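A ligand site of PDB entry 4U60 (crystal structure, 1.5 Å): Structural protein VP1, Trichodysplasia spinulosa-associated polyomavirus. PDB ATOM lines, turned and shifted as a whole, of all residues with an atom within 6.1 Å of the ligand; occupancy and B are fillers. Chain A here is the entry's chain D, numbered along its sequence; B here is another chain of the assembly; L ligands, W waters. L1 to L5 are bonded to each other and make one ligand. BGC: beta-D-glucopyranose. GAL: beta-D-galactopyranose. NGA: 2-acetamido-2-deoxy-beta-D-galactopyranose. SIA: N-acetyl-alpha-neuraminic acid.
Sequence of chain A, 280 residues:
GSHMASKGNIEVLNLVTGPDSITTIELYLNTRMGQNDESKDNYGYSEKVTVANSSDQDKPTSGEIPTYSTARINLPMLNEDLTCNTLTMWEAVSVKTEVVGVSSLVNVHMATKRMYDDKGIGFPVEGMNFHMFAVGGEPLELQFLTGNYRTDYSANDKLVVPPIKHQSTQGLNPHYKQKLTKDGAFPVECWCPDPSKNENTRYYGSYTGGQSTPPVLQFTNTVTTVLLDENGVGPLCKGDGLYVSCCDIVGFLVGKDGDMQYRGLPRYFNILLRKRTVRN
An oxygen (O10) of SIA L4 is in hydrogen-bond range of the backbone NH (N) of Lys 59 (3.0 Å).
O of Lys 59 sits at hydrogen-bond distance from O4 of SIA L4, at 2.5 Å.
A nitrogen (N5) of SIA L4 is in hydrogen-bond range of the side-chain hydroxyl (OG1) of Thr 50 (2.8 Å).
ND2 of Asn 53 is in hydrogen-bond range of O6 of NGA L3 (2.9 Å).
An oxygen (O6) of GAL L5 sits at hydrogen-bond distance from the guanidinium group (NH2) of Arg 114 of chain B, at 3.2 Å.
Water W12 lies within hydrogen-bond range of an oxygen (O8) of SIA L4 (2.6 Å), the guanidinium group (NH2) of Arg 114 of chain B (2.9 Å) and the backbone NH (N) of Val 51 (3.1 Å).
Water W10 lies within hydrogen-bond range of an oxygen (O6) of GAL L5 (2.7 Å) and the guanidinium group of Arg 114 of chain B (2.8 Å).
Water W11 lies within hydrogen-bond range of O of Gln 57 (2.7 Å), O7 of SIA L4 (2.7 Å) and N of Asn 53 (2.9 Å).
Water W7 lies within hydrogen-bond range of O7 of SIA L4 (2.8 Å) and ND2 of Asn 53 (3.5 Å).
Water W6 bridges O10 of SIA L4 (3.0 Å) and O of Gln 57 (3.4 Å).
The backbone carbonyl oxygen (O) of Gln 57 lies close to an oxygen (O10) of SIA L4, at 3.2 Å.
Merely in contact with the ligand: Val 51, Ala 52, Asp 58, Pro 60, Thr 61, His 109 of chain B, Asp 118 of chain B and Lys 119 of chain B.
The nearest printed residue that does not touch the ligand is Lys 48 (4.4 Å).
OG1 of Thr 50 lies within hydrogen-bond range of OE1 of Glu 64 (2.6 Å).
O of Lys 119 of chain B lies within hydrogen-bond range of NH1 of Arg 114 of chain B, at 3.3 Å.
The guanidinium group of Arg 114 of chain B lies close to the backbone carbonyl oxygen of Asp 118 of chain B (3.3 Å).
The side-chain hydroxyl (OG1) of Thr 61 sits at hydrogen-bond distance from the side-chain carboxylate (OE1) of Glu 64, 2.8 Å away.
N of Ala 52 lies within hydrogen-bond range of O of His 109 of chain B (2.9 Å).
O of Ala 52 is in hydrogen-bond range of NZ of Lys 256 of chain B (3.0 Å).
A ring nitrogen (ND1) of His 109 of chain B lies within hydrogen-bond range of the side-chain carboxylate (OD1) of Asp 58, 2.8 Å away.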
ATOM      1  N   LYS A  48     -16.202  18.473  -8.780  1.00  0.00           N
ATOM      2  CA  LYS A  48     -16.506  17.081  -9.097  1.00  0.00           C
ATOM      3  C   LYS A  48     -15.985  16.688 -10.476  1.00  0.00           C
ATOM      4  O   LYS A  48     -16.221  17.386 -11.469  1.00  0.00           O
ATOM      5  CB  LYS A  48     -18.028  16.854  -9.060  1.00  0.00           C
ATOM      6  CG  LYS A  48     -18.493  15.443  -9.399  1.00  0.00           C
ATOM      7  CD  LYS A  48     -19.995  15.240  -9.181  1.00  0.00           C
ATOM      8  CE  LYS A  48     -20.863  15.980 -10.174  1.00  0.00           C
ATOM      9  NZ  LYS A  48     -22.319  15.806  -9.842  1.00  0.00           N
ATOM     10  N   THR A  50     -15.904  14.951 -13.989  1.00  0.00           N
ATOM     11  CA  THR A  50     -16.876  14.466 -14.978  1.00  0.00           C
ATOM     12  C   THR A  50     -16.123  13.672 -16.053  1.00  0.00           C
ATOM     13  O   THR A  50     -14.911  13.765 -16.156  1.00  0.00           O
ATOM     14  CB  THR A  50     -17.681  15.613 -15.628  1.00  0.00           C
ATOM     15  OG1 THR A  50     -16.822  16.418 -16.459  1.00  0.00           O
ATOM     16  CG2 THR A  50     -18.358  16.468 -14.580  1.00  0.00           C
ATOM     17  N   VAL A  51     -16.851  12.878 -16.838  1.00  0.00           N
ATOM     18  CA  VAL A  51     -16.241  11.964 -17.817  1.00  0.00           C
ATOM     19  C   VAL A  51     -16.873  12.205 -19.180  1.00  0.00           C
ATOM     20  O   VAL A  51     -18.119  12.185 -19.347  1.00  0.00           O
ATOM     21  CB  VAL A  51     -16.393  10.504 -17.356  1.00  0.00           C
ATOM     22  CG1 VAL A  51     -15.899   9.497 -18.405  1.00  0.00           C
ATOM     23  CG2 VAL A  51     -15.667  10.309 -16.030  1.00  0.00           C
ATOM     24  N   ALA A  52     -16.015  12.392 -20.176  1.00  0.00           N
ATOM     25  CA  ALA A  52     -16.453  12.636 -21.545  1.00  0.00           C
ATOM     26  C   ALA A  52     -17.271  11.471 -22.096  1.00  0.00           C
ATOM     27  O   ALA A  52     -16.972  10.291 -21.844  1.00  0.00           O
ATOM     28  CB  ALA A  52     -15.248  12.901 -22.437  1.00  0.00           C
ATOM     29  N   ASN A  53     -18.295  11.792 -22.881  1.00  0.00           N
ATOM     30  CA  ASN A  53     -19.066  10.754 -23.575  1.00  0.00           C
ATOM     31  C   ASN A  53     -18.271  10.184 -24.755  1.00  0.00           C
ATOM     32  O   ASN A  53     -18.448   9.021 -25.142  1.00  0.00           O
ATOM     33  CB  ASN A  53     -20.434  11.287 -24.051  1.00  0.00           C
ATOM     34  CG  ASN A  53     -21.447  11.418 -22.927  1.00  0.00           C
ATOM     35  OD1 ASN A  53     -21.393  10.702 -21.915  1.00  0.00           O
ATOM     36  ND2 ASN A  53     -22.399  12.321 -23.097  1.00  0.00           N
ATOM     37  N   GLN A  57     -16.019  15.026 -27.601  1.00  0.00           N
ATOM     38  CA  GLN A  57     -16.887  15.789 -26.705  1.00  0.00           C
ATOM     39  C   GLN A  57     -16.273  15.854 -25.309  1.00  0.00           C
ATOM     40  O   GLN A  57     -16.955  15.575 -24.318  1.00  0.00           O
ATOM     41  CB  GLN A  57     -18.273  15.133 -26.577  1.00  0.00           C
ATOM     42  CG  GLN A  57     -19.107  15.028 -27.832  1.00  0.00           C
ATOM     43  CD  GLN A  57     -20.355  14.201 -27.566  1.00  0.00           C
ATOM     44  OE1 GLN A  57     -20.298  12.966 -27.511  1.00  0.00           O
ATOM     45  NE2 GLN A  57     -21.474  14.876 -27.361  1.00  0.00           N
ATOM     46  N   ASP A  58     -14.980  16.142 -25.233  1.00  0.00           N
ATOM     47  CA  ASP A  58     -14.214  16.047 -23.999  1.00  0.00           C
ATOM     48  C   ASP A  58     -13.945  17.468 -23.503  1.00  0.00           C
ATOM     49  O   ASP A  58     -12.961  18.108 -23.870  1.00  0.00           O
ATOM     50  CB  ASP A  58     -12.915  15.267 -24.250  1.00  0.00           C
ATOM     51  CG  ASP A  58     -12.105  14.982 -22.983  1.00  0.00           C
ATOM     52  OD1 ASP A  58     -12.408  15.509 -21.875  1.00  0.00           O
ATOM     53  OD2 ASP A  58     -11.114  14.227 -23.109  1.00  0.00           O
ATOM     54  N   LYS A  59     -14.867  17.954 -22.676  1.00  0.00           N
ATOM     55  CA  LYS A  59     -14.888  19.341 -22.223  1.00  0.00           C
ATOM     56  C   LYS A  59     -14.987  19.381 -20.698  1.00  0.00           C
ATOM     57  O   LYS A  59     -16.093  19.390 -20.137  1.00  0.00           O
ATOM     58  CB  LYS A  59     -16.075  20.090 -22.837  1.00  0.00           C
ATOM     59  CG  LYS A  59     -16.115  21.566 -22.520  1.00  0.00           C
ATOM     60  CD  LYS A  59     -17.332  22.258 -23.126  1.00  0.00           C
ATOM     61  CE  LYS A  59     -17.237  23.768 -22.908  1.00  0.00           C
ATOM     62  NZ  LYS A  59     -18.325  24.541 -23.556  1.00  0.00           N
ATOM     63  N   PRO A  60     -13.841  19.406 -20.005  1.00  0.00           N
ATOM     64  CA  PRO A  60     -13.910  19.428 -18.531  1.00  0.00           C
ATOM     65  C   PRO A  60     -14.655  20.654 -18.009  1.00  0.00           C
ATOM     66  O   PRO A  60     -14.564  21.748 -18.587  1.00  0.00           O
ATOM     67  CB  PRO A  60     -12.436  19.436 -18.084  1.00  0.00           C
ATOM     68  CG  PRO A  60     -11.647  19.752 -19.313  1.00  0.00           C
ATOM     69  CD  PRO A  60     -12.450  19.349 -20.500  1.00  0.00           C
ATOM     70  N   THR A  61     -15.438  20.443 -16.953  1.00  0.00           N
ATOM     71  CA  THR A  61     -16.128  21.549 -16.310  1.00  0.00           C
ATOM     72  C   THR A  61     -15.115  22.533 -15.703  1.00  0.00           C
ATOM     73  O   THR A  61     -13.956  22.195 -15.446  1.00  0.00           O
ATOM     74  CB  THR A  61     -17.079  21.073 -15.193  1.00  0.00           C
ATOM     75  OG1 THR A  61     -16.349  20.390 -14.182  1.00  0.00           O
ATOM     76  CG2 THR A  61     -18.162  20.168 -15.742  1.00  0.00           C
ATOM     77  N   GLU A  64     -12.567  21.571 -12.481  1.00  0.00           N
ATOM     78  CA  GLU A  64     -12.259  20.157 -12.222  1.00  0.00           C
ATOM     79  C   GLU A  64     -10.842  19.736 -12.600  1.00  0.00           C
ATOM     80  O   GLU A  64     -10.514  18.576 -12.435  1.00  0.00           O
ATOM     81  CB  GLU A  64     -13.275  19.170 -12.854  1.00  0.00           C
ATOM     82  CG  GLU A  64     -13.212  18.971 -14.361  1.00  0.00           C
ATOM     83  CD  GLU A  64     -14.092  17.817 -14.810  1.00  0.00           C
ATOM     84  OE1 GLU A  64     -15.243  18.093 -15.275  1.00  0.00           O
ATOM     85  OE2 GLU A  64     -13.662  16.647 -14.656  1.00  0.00           O
ATOM     86  N   ALA A 155     -14.611  25.907 -21.112  1.00  0.00           N
ATOM     87  CA  ALA A 155     -15.426  26.150 -19.919  1.00  0.00           C
ATOM     88  C   ALA A 155     -14.754  27.112 -18.937  1.00  0.00           C
ATOM     89  O   ALA A 155     -15.424  27.679 -18.061  1.00  0.00           O
ATOM     90  CB  ALA A 155     -15.752  24.837 -19.199  1.00  0.00           C
ATOM     91  N   ASP A 259     -19.241  10.190  -6.426  1.00  0.00           N
ATOM     92  CA  ASP A 259     -18.693  11.420  -7.013  1.00  0.00           C
ATOM     93  C   ASP A 259     -17.295  11.658  -6.438  1.00  0.00           C
ATOM     94  O   ASP A 259     -17.094  11.457  -5.224  1.00  0.00           O
ATOM     95  CB  ASP A 259     -19.560  12.633  -6.660  1.00  0.00           C
ATOM     96  CG  ASP A 259     -21.036  12.452  -7.041  1.00  0.00           C
ATOM     97  OD1 ASP A 259     -21.390  12.568  -8.234  1.00  0.00           O
ATOM     98  OD2 ASP A 259     -21.840  12.205  -6.147  1.00  0.00           O
ATOM     99  N   HIS B 109     -10.885  12.556 -16.948  1.00  0.00           N
ATOM    100  CA  HIS B 109     -12.127  12.991 -17.596  1.00  0.00           C
ATOM    101  C   HIS B 109     -12.236  12.561 -19.064  1.00  0.00           C
ATOM    102  O   HIS B 109     -13.177  12.969 -19.766  1.00  0.00           O
ATOM    103  CB  HIS B 109     -12.326  14.510 -17.448  1.00  0.00           C
ATOM    104  CG  HIS B 109     -11.216  15.325 -18.028  1.00  0.00           C
ATOM    105  ND1 HIS B 109     -11.066  15.526 -19.389  1.00  0.00           N
ATOM    106  CD2 HIS B 109     -10.190  15.958 -17.428  1.00  0.00           C
ATOM    107  CE1 HIS B 109      -9.962  16.225 -19.591  1.00  0.00           C
ATOM    108  NE2 HIS B 109      -9.436  16.527 -18.425  1.00  0.00           N
ATOM    109  N   MET B 110     -11.286  11.747 -19.534  1.00  0.00           N
ATOM    110  CA  MET B 110     -11.349  11.244 -20.901  1.00  0.00           C
ATOM    111  C   MET B 110     -12.488  10.241 -21.017  1.00  0.00           C
ATOM    112  O   MET B 110     -12.988   9.744 -20.003  1.00  0.00           O
ATOM    113  CB  MET B 110     -10.007  10.624 -21.316  1.00  0.00           C
ATOM    114  CG  MET B 110      -8.944  11.682 -21.490  1.00  0.00           C
ATOM    115  SD  MET B 110      -7.421  11.045 -22.202  1.00  0.00           S
ATOM    116  CE  MET B 110      -6.846   9.990 -20.911  1.00  0.00           C
ATOM    117  N   ARG B 114     -15.464   4.110 -16.033  1.00  0.00           N
ATOM    118  CA  ARG B 114     -15.357   4.936 -14.841  1.00  0.00           C
ATOM    119  C   ARG B 114     -15.669   4.160 -13.566  1.00  0.00           C
ATOM    120  O   ARG B 114     -16.280   3.093 -13.589  1.00  0.00           O
ATOM    121  CB  ARG B 114     -16.204   6.219 -14.993  1.00  0.00           C
ATOM    122  CG  ARG B 114     -17.675   6.040 -15.076  1.00  0.00           C
ATOM    123  CD  ARG B 114     -18.392   7.352 -15.463  1.00  0.00           C
ATOM    124  NE  ARG B 114     -18.158   8.440 -14.496  1.00  0.00           N
ATOM    125  CZ  ARG B 114     -18.708   9.652 -14.565  1.00  0.00           C
ATOM    126  NH1 ARG B 114     -18.400  10.553 -13.641  1.00  0.00           N
ATOM    127  NH2 ARG B 114     -19.572   9.965 -15.537  1.00  0.00           N
ATOM    128  N   ASP B 118     -20.700   4.447 -12.434  1.00  0.00           N
ATOM    129  CA  ASP B 118     -20.742   5.564 -13.382  1.00  0.00           C
ATOM    130  C   ASP B 118     -20.797   6.951 -12.757  1.00  0.00           C
ATOM    131  O   ASP B 118     -21.219   7.903 -13.398  1.00  0.00           O
ATOM    132  CB  ASP B 118     -21.892   5.387 -14.384  1.00  0.00           C
ATOM    133  CG  ASP B 118     -21.561   4.417 -15.500  1.00  0.00           C
ATOM    134  OD1 ASP B 118     -20.377   4.128 -15.746  1.00  0.00           O
ATOM    135  OD2 ASP B 118     -22.509   3.931 -16.141  1.00  0.00           O
ATOM    136  N   LYS B 119     -20.365   7.075 -11.501  1.00  0.00           N
ATOM    137  CA  LYS B 119     -20.327   8.346 -10.828  1.00  0.00           C
ATOM    138  C   LYS B 119     -18.925   8.895 -10.587  1.00  0.00           C
ATOM    139  O   LYS B 119     -18.777  10.098 -10.373  1.00  0.00           O
ATOM    140  CB  LYS B 119     -21.014   8.225  -9.461  1.00  0.00           C
ATOM    141  CG  LYS B 119     -22.462   7.823  -9.524  1.00  0.00           C
ATOM    142  CD  LYS B 119     -23.267   8.894 -10.216  1.00  0.00           C
ATOM    143  CE  LYS B 119     -24.720   8.476 -10.358  1.00  0.00           C
ATOM    144  NZ  LYS B 119     -25.556   9.184  -9.366  1.00  0.00           N
ATOM    145  N   LYS B 256     -14.864   3.113 -22.874  1.00  0.00           N
ATOM    146  CA  LYS B 256     -16.173   2.954 -22.264  1.00  0.00           C
ATOM    147  C   LYS B 256     -16.661   1.518 -22.211  1.00  0.00           C
ATOM    148  O   LYS B 256     -17.198   1.077 -21.197  1.00  0.00           O
ATOM    149  CB  LYS B 256     -17.197   3.756 -23.063  1.00  0.00           C
ATOM    150  CG  LYS B 256     -16.958   5.256 -23.050  1.00  0.00           C
ATOM    151  CD  LYS B 256     -17.895   5.919 -22.075  1.00  0.00           C
ATOM    152  CE  LYS B 256     -17.567   7.393 -21.932  1.00  0.00           C
ATOM    153  NZ  LYS B 256     -18.376   7.907 -20.800  1.00  0.00           N
HETATM  154  C2  BGC L   1     -29.031  23.041 -21.484  1.00  0.00           C
HETATM  155  C3  BGC L   1     -28.302  22.280 -20.390  1.00  0.00           C
HETATM  156  C4  BGC L   1     -26.811  22.273 -20.710  1.00  0.00           C
HETATM  157  C5  BGC L   1     -26.313  23.715 -20.848  1.00  0.00           C
HETATM  158  C6  BGC L   1     -24.813  23.803 -21.097  1.00  0.00           C
HETATM  159  C1  BGC L   1     -28.412  24.441 -21.632  1.00  0.00           C
HETATM  160  O1  BGC L   1     -29.072  25.149 -22.690  1.00  0.00           O
HETATM  161  O2  BGC L   1     -30.405  23.189 -21.148  1.00  0.00           O
HETATM  162  O3  BGC L   1     -28.761  20.927 -20.250  1.00  0.00           O
HETATM  163  O4  BGC L   1     -26.152  21.620 -19.623  1.00  0.00           O
HETATM  164  O5  BGC L   1     -27.026  24.299 -21.942  1.00  0.00           O
HETATM  165  O6  BGC L   1     -24.532  23.270 -22.397  1.00  0.00           O
HETATM  166  C1  GAL L   2     -25.288  20.584 -20.108  1.00  0.00           C
HETATM  167  C2  GAL L   2     -24.441  20.152 -18.910  1.00  0.00           C
HETATM  168  C3  GAL L   2     -23.519  19.000 -19.289  1.00  0.00           C
HETATM  169  C4  GAL L   2     -24.330  17.902 -19.977  1.00  0.00           C
HETATM  170  C5  GAL L   2     -25.090  18.502 -21.150  1.00  0.00           C
HETATM  171  C6  GAL L   2     -25.889  17.476 -21.951  1.00  0.00           C
HETATM  172  O2  GAL L   2     -23.639  21.224 -18.484  1.00  0.00           O
HETATM  173  O3  GAL L   2     -22.979  18.559 -18.057  1.00  0.00           O
HETATM  174  O4  GAL L   2     -25.276  17.407 -19.057  1.00  0.00           O
HETATM  175  O5  GAL L   2     -25.992  19.470 -20.616  1.00  0.00           O
HETATM  176  O6  GAL L   2     -26.360  18.146 -23.116  1.00  0.00           O
HETATM  177  C1  NGA L   3     -24.975  16.049 -18.748  1.00  0.00           C
HETATM  178  C2  NGA L   3     -25.510  15.719 -17.377  1.00  0.00           C
HETATM  179  C3  NGA L   3     -25.139  14.283 -17.052  1.00  0.00           C
HETATM  180  C4  NGA L   3     -25.649  13.341 -18.139  1.00  0.00           C
HETATM  181  C5  NGA L   3     -25.133  13.807 -19.500  1.00  0.00           C
HETATM  182  C6  NGA L   3     -25.578  12.969 -20.696  1.00  0.00           C
HETATM  183  C7  NGA L   3     -25.636  17.271 -15.464  1.00  0.00           C
HETATM  184  C8  NGA L   3     -24.856  18.214 -14.584  1.00  0.00           C
HETATM  185  N2  NGA L   3     -24.933  16.665 -16.425  1.00  0.00           N
HETATM  186  O3  NGA L   3     -25.682  13.925 -15.779  1.00  0.00           O
HETATM  187  O4  NGA L   3     -27.085  13.319 -18.113  1.00  0.00           O
HETATM  188  O5  NGA L   3     -25.521  15.172 -19.728  1.00  0.00           O
HETATM  189  O6  NGA L   3     -24.809  13.381 -21.828  1.00  0.00           O
HETATM  190  O7  NGA L   3     -26.821  17.062 -15.304  1.00  0.00           O
HETATM  191  C1  SIA L   4     -21.466  17.841 -16.536  1.00  0.00           C
HETATM  192  C2  SIA L   4     -21.597  18.135 -18.025  1.00  0.00           C
HETATM  193  C3  SIA L   4     -20.604  19.211 -18.514  1.00  0.00           C
HETATM  194  C4  SIA L   4     -19.164  18.705 -18.694  1.00  0.00           C
HETATM  195  C5  SIA L   4     -19.069  17.311 -19.335  1.00  0.00           C
HETATM  196  C6  SIA L   4     -20.098  16.376 -18.697  1.00  0.00           C
HETATM  197  C7  SIA L   4     -20.151  14.971 -19.296  1.00  0.00           C
HETATM  198  C8  SIA L   4     -21.296  14.158 -18.671  1.00  0.00           C
HETATM  199  C9  SIA L   4     -21.211  12.682 -19.031  1.00  0.00           C
HETATM  200  C10 SIA L   4     -16.858  16.431 -20.089  1.00  0.00           C
HETATM  201  C11 SIA L   4     -15.499  15.925 -19.645  1.00  0.00           C
HETATM  202  N5  SIA L   4     -17.711  16.798 -19.123  1.00  0.00           N
HETATM  203  O1A SIA L   4     -21.112  18.736 -15.738  1.00  0.00           O
HETATM  204  O1B SIA L   4     -21.802  16.689 -16.141  1.00  0.00           O
HETATM  205  O4  SIA L   4     -18.425  19.702 -19.431  1.00  0.00           O
HETATM  206  O6  SIA L   4     -21.437  16.940 -18.795  1.00  0.00           O
HETATM  207  O7  SIA L   4     -20.373  15.128 -20.705  1.00  0.00           O
HETATM  208  O8  SIA L   4     -21.340  14.279 -17.233  1.00  0.00           O
HETATM  209  O9  SIA L   4     -22.430  12.004 -18.668  1.00  0.00           O
HETATM  210  O10 SIA L   4     -17.108  16.521 -21.283  1.00  0.00           O
HETATM  211  C1  GAL L   5     -24.665  13.340 -14.939  1.00  0.00           C
HETATM  212  C2  GAL L   5     -25.221  13.283 -13.529  1.00  0.00           C
HETATM  213  C3  GAL L   5     -24.239  12.576 -12.594  1.00  0.00           C
HETATM  214  C4  GAL L   5     -23.809  11.238 -13.185  1.00  0.00           C
HETATM  215  C5  GAL L   5     -23.305  11.435 -14.627  1.00  0.00           C
HETATM  216  C6  GAL L   5     -22.931  10.130 -15.324  1.00  0.00           C
HETATM  217  O2  GAL L   5     -25.455  14.603 -13.091  1.00  0.00           O
HETATM  218  O3  GAL L   5     -24.814  12.431 -11.300  1.00  0.00           O
HETATM  219  O4  GAL L   5     -24.891  10.326 -13.132  1.00  0.00           O
HETATM  220  O5  GAL L   5     -24.296  12.062 -15.407  1.00  0.00           O
HETATM  221  O6  GAL L   5     -22.492  10.440 -16.638  1.00  0.00           O
HETATM  222  O   HOH W   1     -20.506  18.731 -12.762  1.00  0.00           O
HETATM  223  O   HOH W   2     -21.608  15.091 -13.794  1.00  0.00           O
HETATM  224  O   HOH W   3     -19.073  22.491 -18.833  1.00  0.00           O
HETATM  225  O   HOH W   4     -28.487  23.537 -25.215  1.00  0.00           O
HETATM  226  O   HOH W   5     -19.706   9.935 -19.793  1.00  0.00           O
HETATM  227  O   HOH W   6     -19.158  17.755 -23.009  1.00  0.00           O
HETATM  228  O   HOH W   7     -22.914  15.487 -21.822  1.00  0.00           O
HETATM  229  O   HOH W   8     -32.130  24.236 -22.734  1.00  0.00           O
HETATM  230  O   HOH W   9     -30.953  23.548 -18.517  1.00  0.00           O
HETATM  231  O   HOH W  10     -20.797   8.627 -17.666  1.00  0.00           O
HETATM  232  O   HOH W  11     -19.130  14.577 -23.058  1.00  0.00           O
HETATM  233  O   HOH W  12     -19.770  12.835 -15.738  1.00  0.00           O
